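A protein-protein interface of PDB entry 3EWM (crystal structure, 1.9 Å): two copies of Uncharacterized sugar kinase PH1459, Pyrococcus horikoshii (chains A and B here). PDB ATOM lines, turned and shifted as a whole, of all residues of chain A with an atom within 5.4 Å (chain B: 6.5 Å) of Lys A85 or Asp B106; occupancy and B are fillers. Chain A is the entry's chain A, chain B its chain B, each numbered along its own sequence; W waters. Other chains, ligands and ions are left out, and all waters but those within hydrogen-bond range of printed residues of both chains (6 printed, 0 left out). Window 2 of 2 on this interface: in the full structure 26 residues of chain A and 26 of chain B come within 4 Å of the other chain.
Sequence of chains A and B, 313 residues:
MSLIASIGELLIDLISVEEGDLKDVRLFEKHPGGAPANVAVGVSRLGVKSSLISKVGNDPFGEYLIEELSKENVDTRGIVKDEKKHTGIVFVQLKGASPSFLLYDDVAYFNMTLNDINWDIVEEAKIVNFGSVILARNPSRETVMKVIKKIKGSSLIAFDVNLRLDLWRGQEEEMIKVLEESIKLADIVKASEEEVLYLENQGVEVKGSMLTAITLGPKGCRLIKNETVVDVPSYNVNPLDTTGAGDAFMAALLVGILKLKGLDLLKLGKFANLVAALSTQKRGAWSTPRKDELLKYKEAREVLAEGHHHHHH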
ATOM      1  N   VAL A  56     -31.038  14.941  14.640  1.00  0.00           N
ATOM      2  CA  VAL A  56     -31.089  15.842  13.476  1.00  0.00           C
ATOM      3  C   VAL A  56     -29.688  15.917  12.891  1.00  0.00           C
ATOM      4  O   VAL A  56     -28.731  15.403  13.480  1.00  0.00           O
ATOM      5  CB  VAL A  56     -31.596  17.266  13.861  1.00  0.00           C
ATOM      6  CG1 VAL A  56     -33.062  17.225  14.294  1.00  0.00           C
ATOM      7  CG2 VAL A  56     -30.735  17.878  14.964  1.00  0.00           C
ATOM      8  N   GLY A  57     -29.565  16.555  11.735  1.00  0.00           N
ATOM      9  CA  GLY A  57     -28.268  16.775  11.139  1.00  0.00           C
ATOM     10  C   GLY A  57     -27.609  17.938  11.850  1.00  0.00           C
ATOM     11  O   GLY A  57     -28.279  18.835  12.381  1.00  0.00           O
ATOM     12  N   ASN A  58     -26.286  17.927  11.852  1.00  0.00           N
ATOM     13  CA  ASN A  58     -25.530  19.115  12.236  1.00  0.00           C
ATOM     14  C   ASN A  58     -25.611  20.106  11.072  1.00  0.00           C
ATOM     15  O   ASN A  58     -24.682  20.268  10.284  1.00  0.00           O
ATOM     16  CB  ASN A  58     -24.078  18.760  12.590  1.00  0.00           C
ATOM     17  CG  ASN A  58     -23.258  19.985  12.968  1.00  0.00           C
ATOM     18  OD1 ASN A  58     -23.806  21.040  13.338  1.00  0.00           O
ATOM     19  ND2 ASN A  58     -21.932  19.855  12.879  1.00  0.00           N
ATOM     20  N   ASP A  59     -26.767  20.734  10.953  1.00  0.00           N
ATOM     21  CA  ASP A  59     -27.060  21.609   9.834  1.00  0.00           C
ATOM     22  C   ASP A  59     -28.083  22.658  10.258  1.00  0.00           C
ATOM     23  O   ASP A  59     -28.620  22.573  11.366  1.00  0.00           O
ATOM     24  CB  ASP A  59     -27.455  20.801   8.586  1.00  0.00           C
ATOM     25  CG  ASP A  59     -28.665  19.886   8.793  1.00  0.00           C
ATOM     26  OD1 ASP A  59     -29.688  20.327   9.344  1.00  0.00           O
ATOM     27  OD2 ASP A  59     -28.595  18.722   8.339  1.00  0.00           O
ATOM     28  N   ASP A  82     -26.366  14.544  14.171  1.00  0.00           N
ATOM     29  CA  ASP A  82     -25.690  13.584  13.329  1.00  0.00           C
ATOM     30  C   ASP A  82     -24.716  14.323  12.417  1.00  0.00           C
ATOM     31  O   ASP A  82     -25.093  15.230  11.673  1.00  0.00           O
ATOM     32  CB  ASP A  82     -26.726  12.814  12.520  1.00  0.00           C
ATOM     33  CG  ASP A  82     -26.185  11.526  11.955  1.00  0.00           C
ATOM     34  OD1 ASP A  82     -25.028  11.511  11.484  1.00  0.00           O
ATOM     35  OD2 ASP A  82     -26.938  10.539  11.948  1.00  0.00           O
ATOM     36  N   GLU A  83     -23.445  13.952  12.520  1.00  0.00           N
ATOM     37  CA  GLU A  83     -22.417  14.525  11.663  1.00  0.00           C
ATOM     38  C   GLU A  83     -22.371  13.871  10.285  1.00  0.00           C
ATOM     39  O   GLU A  83     -21.699  14.368   9.386  1.00  0.00           O
ATOM     40  CB  GLU A  83     -21.047  14.412  12.354  1.00  0.00           C
ATOM     41  CG  GLU A  83     -20.975  15.145  13.697  1.00  0.00           C
ATOM     42  CD  GLU A  83     -21.104  16.658  13.566  1.00  0.00           C
ATOM     43  OE1 GLU A  83     -20.926  17.193  12.447  1.00  0.00           O
ATOM     44  OE2 GLU A  83     -21.378  17.316  14.591  1.00  0.00           O
ATOM     45  N   LYS A  84     -23.073  12.758  10.115  1.00  0.00           N
ATOM     46  CA  LYS A  84     -23.039  12.035   8.845  1.00  0.00           C
ATOM     47  C   LYS A  84     -24.362  12.030   8.063  1.00  0.00           C
ATOM     48  O   LYS A  84     -24.387  11.618   6.908  1.00  0.00           O
ATOM     49  CB  LYS A  84     -22.574  10.593   9.055  1.00  0.00           C
ATOM     50  CG  LYS A  84     -21.232  10.452   9.770  1.00  0.00           C
ATOM     51  CD  LYS A  84     -20.109  10.888   8.881  1.00  0.00           C
ATOM     52  CE  LYS A  84     -18.762  10.549   9.511  1.00  0.00           C
ATOM     53  NZ  LYS A  84     -17.667  11.304   8.835  1.00  0.00           N
ATOM     54  N   LYS A  85     -25.458  12.447   8.686  1.00  0.00           N
ATOM     55  CA  LYS A  85     -26.738  12.434   7.990  1.00  0.00           C
ATOM     56  C   LYS A  85     -27.351  13.806   8.155  1.00  0.00           C
ATOM     57  O   LYS A  85     -27.101  14.480   9.134  1.00  0.00           O
ATOM     58  CB  LYS A  85     -27.695  11.351   8.514  1.00  0.00           C
ATOM     59  CG  LYS A  85     -27.167   9.900   8.513  1.00  0.00           C
ATOM     60  CD  LYS A  85     -26.918   9.344   7.137  1.00  0.00           C
ATOM     61  CE  LYS A  85     -26.434   7.883   7.216  1.00  0.00           C
ATOM     62  NZ  LYS A  85     -26.355   7.303   5.843  1.00  0.00           N
ATOM     63  N   HIS A  86     -28.116  14.226   7.162  1.00  0.00           N
ATOM     64  CA  HIS A  86     -28.776  15.516   7.217  1.00  0.00           C
ATOM     65  C   HIS A  86     -30.093  15.386   7.949  1.00  0.00           C
ATOM     66  O   HIS A  86     -30.628  14.290   8.103  1.00  0.00           O
ATOM     67  CB  HIS A  86     -28.961  16.067   5.808  1.00  0.00           C
ATOM     68  CG  HIS A  86     -27.657  16.285   5.117  1.00  0.00           C
ATOM     69  ND1 HIS A  86     -27.196  15.461   4.112  1.00  0.00           N
ATOM     70  CD2 HIS A  86     -26.660  17.163   5.374  1.00  0.00           C
ATOM     71  CE1 HIS A  86     -25.989  15.856   3.747  1.00  0.00           C
ATOM     72  NE2 HIS A  86     -25.642  16.887   4.499  1.00  0.00           N
ATOM     73  N   THR A  87     -30.575  16.525   8.412  1.00  0.00           N
ATOM     74  CA  THR A  87     -31.831  16.612   9.109  1.00  0.00           C
ATOM     75  C   THR A  87     -32.952  16.046   8.241  1.00  0.00           C
ATOM     76  O   THR A  87     -33.005  16.286   7.032  1.00  0.00           O
ATOM     77  CB  THR A  87     -32.100  18.078   9.459  1.00  0.00           C
ATOM     78  OG1 THR A  87     -31.094  18.531  10.384  1.00  0.00           O
ATOM     79  CG2 THR A  87     -33.461  18.237  10.080  1.00  0.00           C
ATOM     80  N   ASP A 106     -32.921   8.661   4.066  1.00  0.00           N
ATOM     81  CA  ASP A 106     -31.585   8.511   4.606  1.00  0.00           C
ATOM     82  C   ASP A 106     -31.202   9.790   5.275  1.00  0.00           C
ATOM     83  O   ASP A 106     -30.429  10.594   4.729  1.00  0.00           O
ATOM     84  CB  ASP A 106     -30.541   8.066   3.597  1.00  0.00           C
ATOM     85  CG  ASP A 106     -29.618   7.036   4.195  1.00  0.00           C
ATOM     86  OD1 ASP A 106     -29.674   5.862   3.753  1.00  0.00           O
ATOM     87  OD2 ASP A 106     -28.905   7.374   5.167  1.00  0.00           O
ATOM     88  N   VAL A 107     -31.787   9.965   6.453  1.00  0.00           N
ATOM     89  CA  VAL A 107     -31.707  11.194   7.199  1.00  0.00           C
ATOM     90  C   VAL A 107     -31.418  10.849   8.658  1.00  0.00           C
ATOM     91  O   VAL A 107     -31.478   9.684   9.060  1.00  0.00           O
ATOM     92  CB  VAL A 107     -33.026  12.003   7.098  1.00  0.00           C
ATOM     93  CG1 VAL A 107     -33.229  12.555   5.661  1.00  0.00           C
ATOM     94  CG2 VAL A 107     -34.216  11.148   7.549  1.00  0.00           C
ATOM     95  N   ALA A 108     -31.136  11.884   9.438  1.00  0.00           N
ATOM     96  CA  ALA A 108     -30.539  11.727  10.747  1.00  0.00           C
ATOM     97  C   ALA A 108     -31.430  10.978  11.726  1.00  0.00           C
ATOM     98  O   ALA A 108     -30.923  10.160  12.506  1.00  0.00           O
ATOM     99  CB  ALA A 108     -30.160  13.079  11.303  1.00  0.00           C
ATOM    100  N   ASN A 111     -31.109   7.349  11.881  1.00  0.00           N
ATOM    101  CA  ASN A 111     -29.754   6.907  12.206  1.00  0.00           C
ATOM    102  C   ASN A 111     -29.430   6.881  13.718  1.00  0.00           C
ATOM    103  O   ASN A 111     -28.278   7.071  14.115  1.00  0.00           O
ATOM    104  CB  ASN A 111     -28.756   7.824  11.485  1.00  0.00           C
ATOM    105  CG  ASN A 111     -27.407   7.172  11.260  1.00  0.00           C
ATOM    106  OD1 ASN A 111     -27.311   5.953  11.071  1.00  0.00           O
ATOM    107  ND2 ASN A 111     -26.359   7.989  11.234  1.00  0.00           N
ATOM    108  N   LYS B  85     -33.021   5.381  -3.922  1.00  0.00           N
ATOM    109  CA  LYS B  85     -32.606   6.716  -3.522  1.00  0.00           C
ATOM    110  C   LYS B  85     -33.586   7.732  -4.086  1.00  0.00           C
ATOM    111  O   LYS B  85     -34.093   7.572  -5.185  1.00  0.00           O
ATOM    112  CB  LYS B  85     -31.195   7.043  -4.034  1.00  0.00           C
ATOM    113  CG  LYS B  85     -30.067   6.083  -3.645  1.00  0.00           C
ATOM    114  CD  LYS B  85     -29.810   6.068  -2.180  1.00  0.00           C
ATOM    115  CE  LYS B  85     -28.706   5.094  -1.834  1.00  0.00           C
ATOM    116  NZ  LYS B  85     -28.392   5.197  -0.402  1.00  0.00           N
ATOM    117  N   HIS B  86     -33.822   8.791  -3.323  1.00  0.00           N
ATOM    118  CA  HIS B  86     -34.691   9.862  -3.743  1.00  0.00           C
ATOM    119  C   HIS B  86     -33.942  10.913  -4.532  1.00  0.00           C
ATOM    120  O   HIS B  86     -32.730  11.013  -4.454  1.00  0.00           O
ATOM    121  CB  HIS B  86     -35.353  10.495  -2.532  1.00  0.00           C
ATOM    122  CG  HIS B  86     -36.217   9.540  -1.788  1.00  0.00           C
ATOM    123  ND1 HIS B  86     -35.890   9.062  -0.535  1.00  0.00           N
ATOM    124  CD2 HIS B  86     -37.354   8.906  -2.157  1.00  0.00           C
ATOM    125  CE1 HIS B  86     -36.821   8.212  -0.145  1.00  0.00           C
ATOM    126  NE2 HIS B  86     -37.722   8.103  -1.108  1.00  0.00           N
ATOM    127  N   LEU B 103     -27.016  20.738   0.908  1.00  0.00           N
ATOM    128  CA  LEU B 103     -27.175  19.734  -0.120  1.00  0.00           C
ATOM    129  C   LEU B 103     -27.301  18.357   0.519  1.00  0.00           C
ATOM    130  O   LEU B 103     -26.454  17.954   1.324  1.00  0.00           O
ATOM    131  CB  LEU B 103     -25.994  19.788  -1.103  1.00  0.00           C
ATOM    132  CG  LEU B 103     -25.940  18.723  -2.210  1.00  0.00           C
ATOM    133  CD1 LEU B 103     -25.288  19.299  -3.453  1.00  0.00           C
ATOM    134  CD2 LEU B 103     -25.213  17.452  -1.782  1.00  0.00           C
ATOM    135  N   TYR B 104     -28.336  17.631   0.111  1.00  0.00           N
ATOM    136  CA  TYR B 104     -28.615  16.301   0.632  1.00  0.00           C
ATOM    137  C   TYR B 104     -27.851  15.333  -0.233  1.00  0.00           C
ATOM    138  O   TYR B 104     -28.102  15.235  -1.429  1.00  0.00           O
ATOM    139  CB  TYR B 104     -30.127  16.012   0.628  1.00  0.00           C
ATOM    140  CG  TYR B 104     -30.745  16.606   1.870  1.00  0.00           C
ATOM    141  CD1 TYR B 104     -30.747  17.992   2.075  1.00  0.00           C
ATOM    142  CD2 TYR B 104     -31.242  15.789   2.874  1.00  0.00           C
ATOM    143  CE1 TYR B 104     -31.265  18.541   3.239  1.00  0.00           C
ATOM    144  CE2 TYR B 104     -31.766  16.320   4.027  1.00  0.00           C
ATOM    145  CZ  TYR B 104     -31.756  17.699   4.217  1.00  0.00           C
ATOM    146  OH  TYR B 104     -32.252  18.244   5.365  1.00  0.00           O
ATOM    147  N   ASP B 105     -26.870  14.678   0.372  1.00  0.00           N
ATOM    148  CA  ASP B 105     -25.905  13.911  -0.399  1.00  0.00           C
ATOM    149  C   ASP B 105     -26.345  12.472  -0.605  1.00  0.00           C
ATOM    150  O   ASP B 105     -25.855  11.811  -1.533  1.00  0.00           O
ATOM    151  CB  ASP B 105     -24.505  13.982   0.239  1.00  0.00           C
ATOM    152  CG  ASP B 105     -24.446  13.266   1.592  1.00  0.00           C
ATOM    153  OD1 ASP B 105     -25.482  13.234   2.269  1.00  0.00           O
ATOM    154  OD2 ASP B 105     -23.378  12.729   1.969  1.00  0.00           O
ATOM    155  N   ASP B 106     -27.237  11.956   0.243  1.00  0.00           N
ATOM    156  CA  ASP B 106     -27.628  10.542   0.066  1.00  0.00           C
ATOM    157  C   ASP B 106     -28.840  10.467  -0.843  1.00  0.00           C
ATOM    158  O   ASP B 106     -29.974  10.236  -0.404  1.00  0.00           O
ATOM    159  CB  ASP B 106     -27.858   9.799   1.380  1.00  0.00           C
ATOM    160  CG  ASP B 106     -27.699   8.290   1.222  1.00  0.00           C
ATOM    161  OD1 ASP B 106     -27.714   7.571   2.249  1.00  0.00           O
ATOM    162  OD2 ASP B 106     -27.544   7.807   0.068  1.00  0.00           O
ATOM    163  N   VAL B 107     -28.566  10.681  -2.122  1.00  0.00           N
ATOM    164  CA  VAL B 107     -29.590  10.948  -3.124  1.00  0.00           C
ATOM    165  C   VAL B 107     -29.183  10.272  -4.425  1.00  0.00           C
ATOM    166  O   VAL B 107     -28.053   9.773  -4.563  1.00  0.00           O
ATOM    167  CB  VAL B 107     -29.839  12.475  -3.342  1.00  0.00           C
ATOM    168  CG1 VAL B 107     -30.472  13.109  -2.107  1.00  0.00           C
ATOM    169  CG2 VAL B 107     -28.547  13.214  -3.746  1.00  0.00           C
ATOM    170  N   ALA B 108     -30.120  10.238  -5.357  1.00  0.00           N
ATOM    171  CA  ALA B 108     -30.033   9.375  -6.519  1.00  0.00           C
ATOM    172  C   ALA B 108     -28.852   9.666  -7.443  1.00  0.00           C
ATOM    173  O   ALA B 108     -28.178   8.745  -7.927  1.00  0.00           O
ATOM    174  CB  ALA B 108     -31.357   9.435  -7.291  1.00  0.00           C
ATOM    175  N   PHE B 110     -25.961  10.694  -6.819  1.00  0.00           N
ATOM    176  CA  PHE B 110     -24.689  10.237  -6.254  1.00  0.00           C
ATOM    177  C   PHE B 110     -24.588   8.713  -6.253  1.00  0.00           C
ATOM    178  O   PHE B 110     -23.567   8.161  -5.833  1.00  0.00           O
ATOM    179  CB  PHE B 110     -24.487  10.749  -4.827  1.00  0.00           C
ATOM    180  CG  PHE B 110     -23.936  12.143  -4.751  1.00  0.00           C
ATOM    181  CD1 PHE B 110     -22.828  12.494  -5.491  1.00  0.00           C
ATOM    182  CD2 PHE B 110     -24.524  13.102  -3.929  1.00  0.00           C
ATOM    183  CE1 PHE B 110     -22.296  13.773  -5.433  1.00  0.00           C
ATOM    184  CE2 PHE B 110     -23.988  14.391  -3.842  1.00  0.00           C
ATOM    185  CZ  PHE B 110     -22.866  14.727  -4.605  1.00  0.00           C
ATOM    186  N   ASN B 111     -25.646   8.060  -6.729  1.00  0.00           N
ATOM    187  CA  ASN B 111     -25.745   6.598  -6.722  1.00  0.00           C
ATOM    188  C   ASN B 111     -25.676   5.977  -8.124  1.00  0.00           C
ATOM    189  O   ASN B 111     -26.255   4.913  -8.390  1.00  0.00           O
ATOM    190  CB  ASN B 111     -27.019   6.176  -5.970  1.00  0.00           C
ATOM    191  CG  ASN B 111     -27.028   4.707  -5.609  1.00  0.00           C
ATOM    192  OD1 ASN B 111     -25.999   4.133  -5.232  1.00  0.00           O
ATOM    193  ND2 ASN B 111     -28.189   4.091  -5.731  1.00  0.00           N
ATOM    194  N   ARG B 137     -19.184  12.013  -4.254  1.00  0.00           N
ATOM    195  CA  ARG B 137     -19.537  10.727  -3.661  1.00  0.00           C
ATOM    196  C   ARG B 137     -19.456   9.581  -4.641  1.00  0.00           C
ATOM    197  O   ARG B 137     -19.726   9.739  -5.831  1.00  0.00           O
ATOM    198  CB  ARG B 137     -20.971  10.734  -3.111  1.00  0.00           C
ATOM    199  CG  ARG B 137     -21.285  11.832  -2.138  1.00  0.00           C
ATOM    200  CD  ARG B 137     -20.722  11.552  -0.731  1.00  0.00           C
ATOM    201  NE  ARG B 137     -21.169  12.600   0.187  1.00  0.00           N
ATOM    202  CZ  ARG B 137     -20.567  13.775   0.355  1.00  0.00           C
ATOM    203  NH1 ARG B 137     -19.458  14.075  -0.315  1.00  0.00           N
ATOM    204  NH2 ARG B 137     -21.085  14.662   1.196  1.00  0.00           N
HETATM  205  O   HOH W   1     -28.923  13.165   2.244  1.00  0.00           O
HETATM  206  O   HOH W   2     -31.199  11.872   1.850  1.00  0.00           O
HETATM  207  O   HOH W   3     -23.735  17.111   1.863  1.00  0.00           O
HETATM  208  O   HOH W   4     -30.600   6.249   1.155  1.00  0.00           O
HETATM  209  O   HOH W   5     -25.825   9.169   3.890  1.00  0.00           O
HETATM  210  O   HOH W   6     -25.819  11.720   4.444  1.00  0.00           O
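Water W6 lies within hydrogen-bond range of OD1 of Asp B105 (2.7 Å) and O of Lys A84 (2.9 Å).
Water W5 bridges NZ of Lys A85 (2.8 Å) and OD1 of Asp B106 (3.0 Å).
Water W4 lies within hydrogen-bond range of the side-chain carboxylate (OD1) of Asp A106 (2.8 Å), the side-chain amino group (NZ) of Lys B85 (2.9 Å) and the side-chain carboxylate (OD1) of Asp B106 (3.4 Å).
Water W1 lies within hydrogen-bond range of the backbone NH of Asp B106, the backbone NH of Asp B105 and a ring nitrogen (ND1) of His A86.
Water W3 lies within hydrogen-bond range of O of Leu B103 (2.9 Å) and NE2 of His A86 (3.3 Å).
Water W2 bridges the backbone carbonyl oxygen of Asp B106 (3.0 Å) and the backbone carbonyl oxygen of Asp A106 (3.2 Å).
Among the printed residues, pairs that only touch across the chains: His A86 with Tyr B104 (3.3 Å).
The side-chain hydroxyl (OH) of Tyr B104 sits at hydrogen-bond distance from the backbone carbonyl oxygen (O) of Thr A87, 2.7 Å away.
A ring nitrogen (ND1) of His A86 sits close to the side-chain carboxylate (OD1) of Asp B105 (3.4 Å).
The side-chain carboxylate (OD1) of Asp A106 sits close to the side-chain carboxylate (OD1) of Asp B106 (3.0 Å).
NE2 of His A86 sits close to O of Leu B103 (3.4 Å).
NZ of Lys A85 lies within salt-bridge range of OD1 of Asp B106, at 3.9 Å.
Lys A85 touches Asp B106, but with the chains exchanged Asp A106 does not touch Lys B85 (4.4 Å).
Asp B106 touches its own counterpart, Asp A106.
Of the 11 printed residues of chain B, 4 touch a printed residue of chain A.
Along chain B the printed residues that touch a printed residue of chain A span positions 103 to 106.
Of the 14 printed residues of chain A, 4 touch a printed residue of chain B.
Printed residues of chain A that touch a printed residue of chain B: Lys A85, His A86, Thr A87 and Asp A106.
Hydrophobic or aromatic side chains of chain A that line the printed part of chain B: His A86.
Among the printed residues, Asp or Glu carboxylates within 4 Å of a Lys or Arg side-chain nitrogen of the other chain: Lys A85 with Asp B106 (3.9 Å).
OD1 of Asp A82 lies within hydrogen-bond range of N of Lys A85, 3.0 Å away.
N of Gly A57 is in hydrogen-bond range of OG1 of Thr A87 (2.8 Å).
The side-chain carboxylate of Asp A59 is in hydrogen-bond range of the side-chain hydroxyl of Thr A87, at 2.5 Å.
The backbone carbonyl oxygen (O) of His A86 lies within hydrogen-bond range of the backbone NH (N) of Ala A108 (2.8 Å).
The side-chain amino group of Lys B85 is in salt-bridge range of the side-chain carboxylate of Asp B106 (2.8 Å).
NE of Arg B137 lies within salt-bridge range of OD2 of Asp B105, 2.8 Å away.
Lys A85 touches just one residue of chain B: Asp B106.
Of chain A, only Lys A85 (3.9 Å) and Asp A106 (2.8 Å) come within 4 Å of Asp B106.
Of the printed residues of chain A, Tyr B104 touches His A86 and Thr A87.
Of the printed residues of chain B, Asp A106 touches Asp B106 (2.8 Å).
Asn A111 touches none of the printed residues of chain B.
Phe B110 touches none of the printed residues of chain A.
The nearest residue of chain B that does not touch Lys A85 is Asp B105 (5.9 Å).
The nearest residue of chain A that does not touch Asp B106 is His A86 (5.2 Å).
The nearest printed residue of chain A that does not touch Leu B103 is Asp A59 (7.4 Å).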
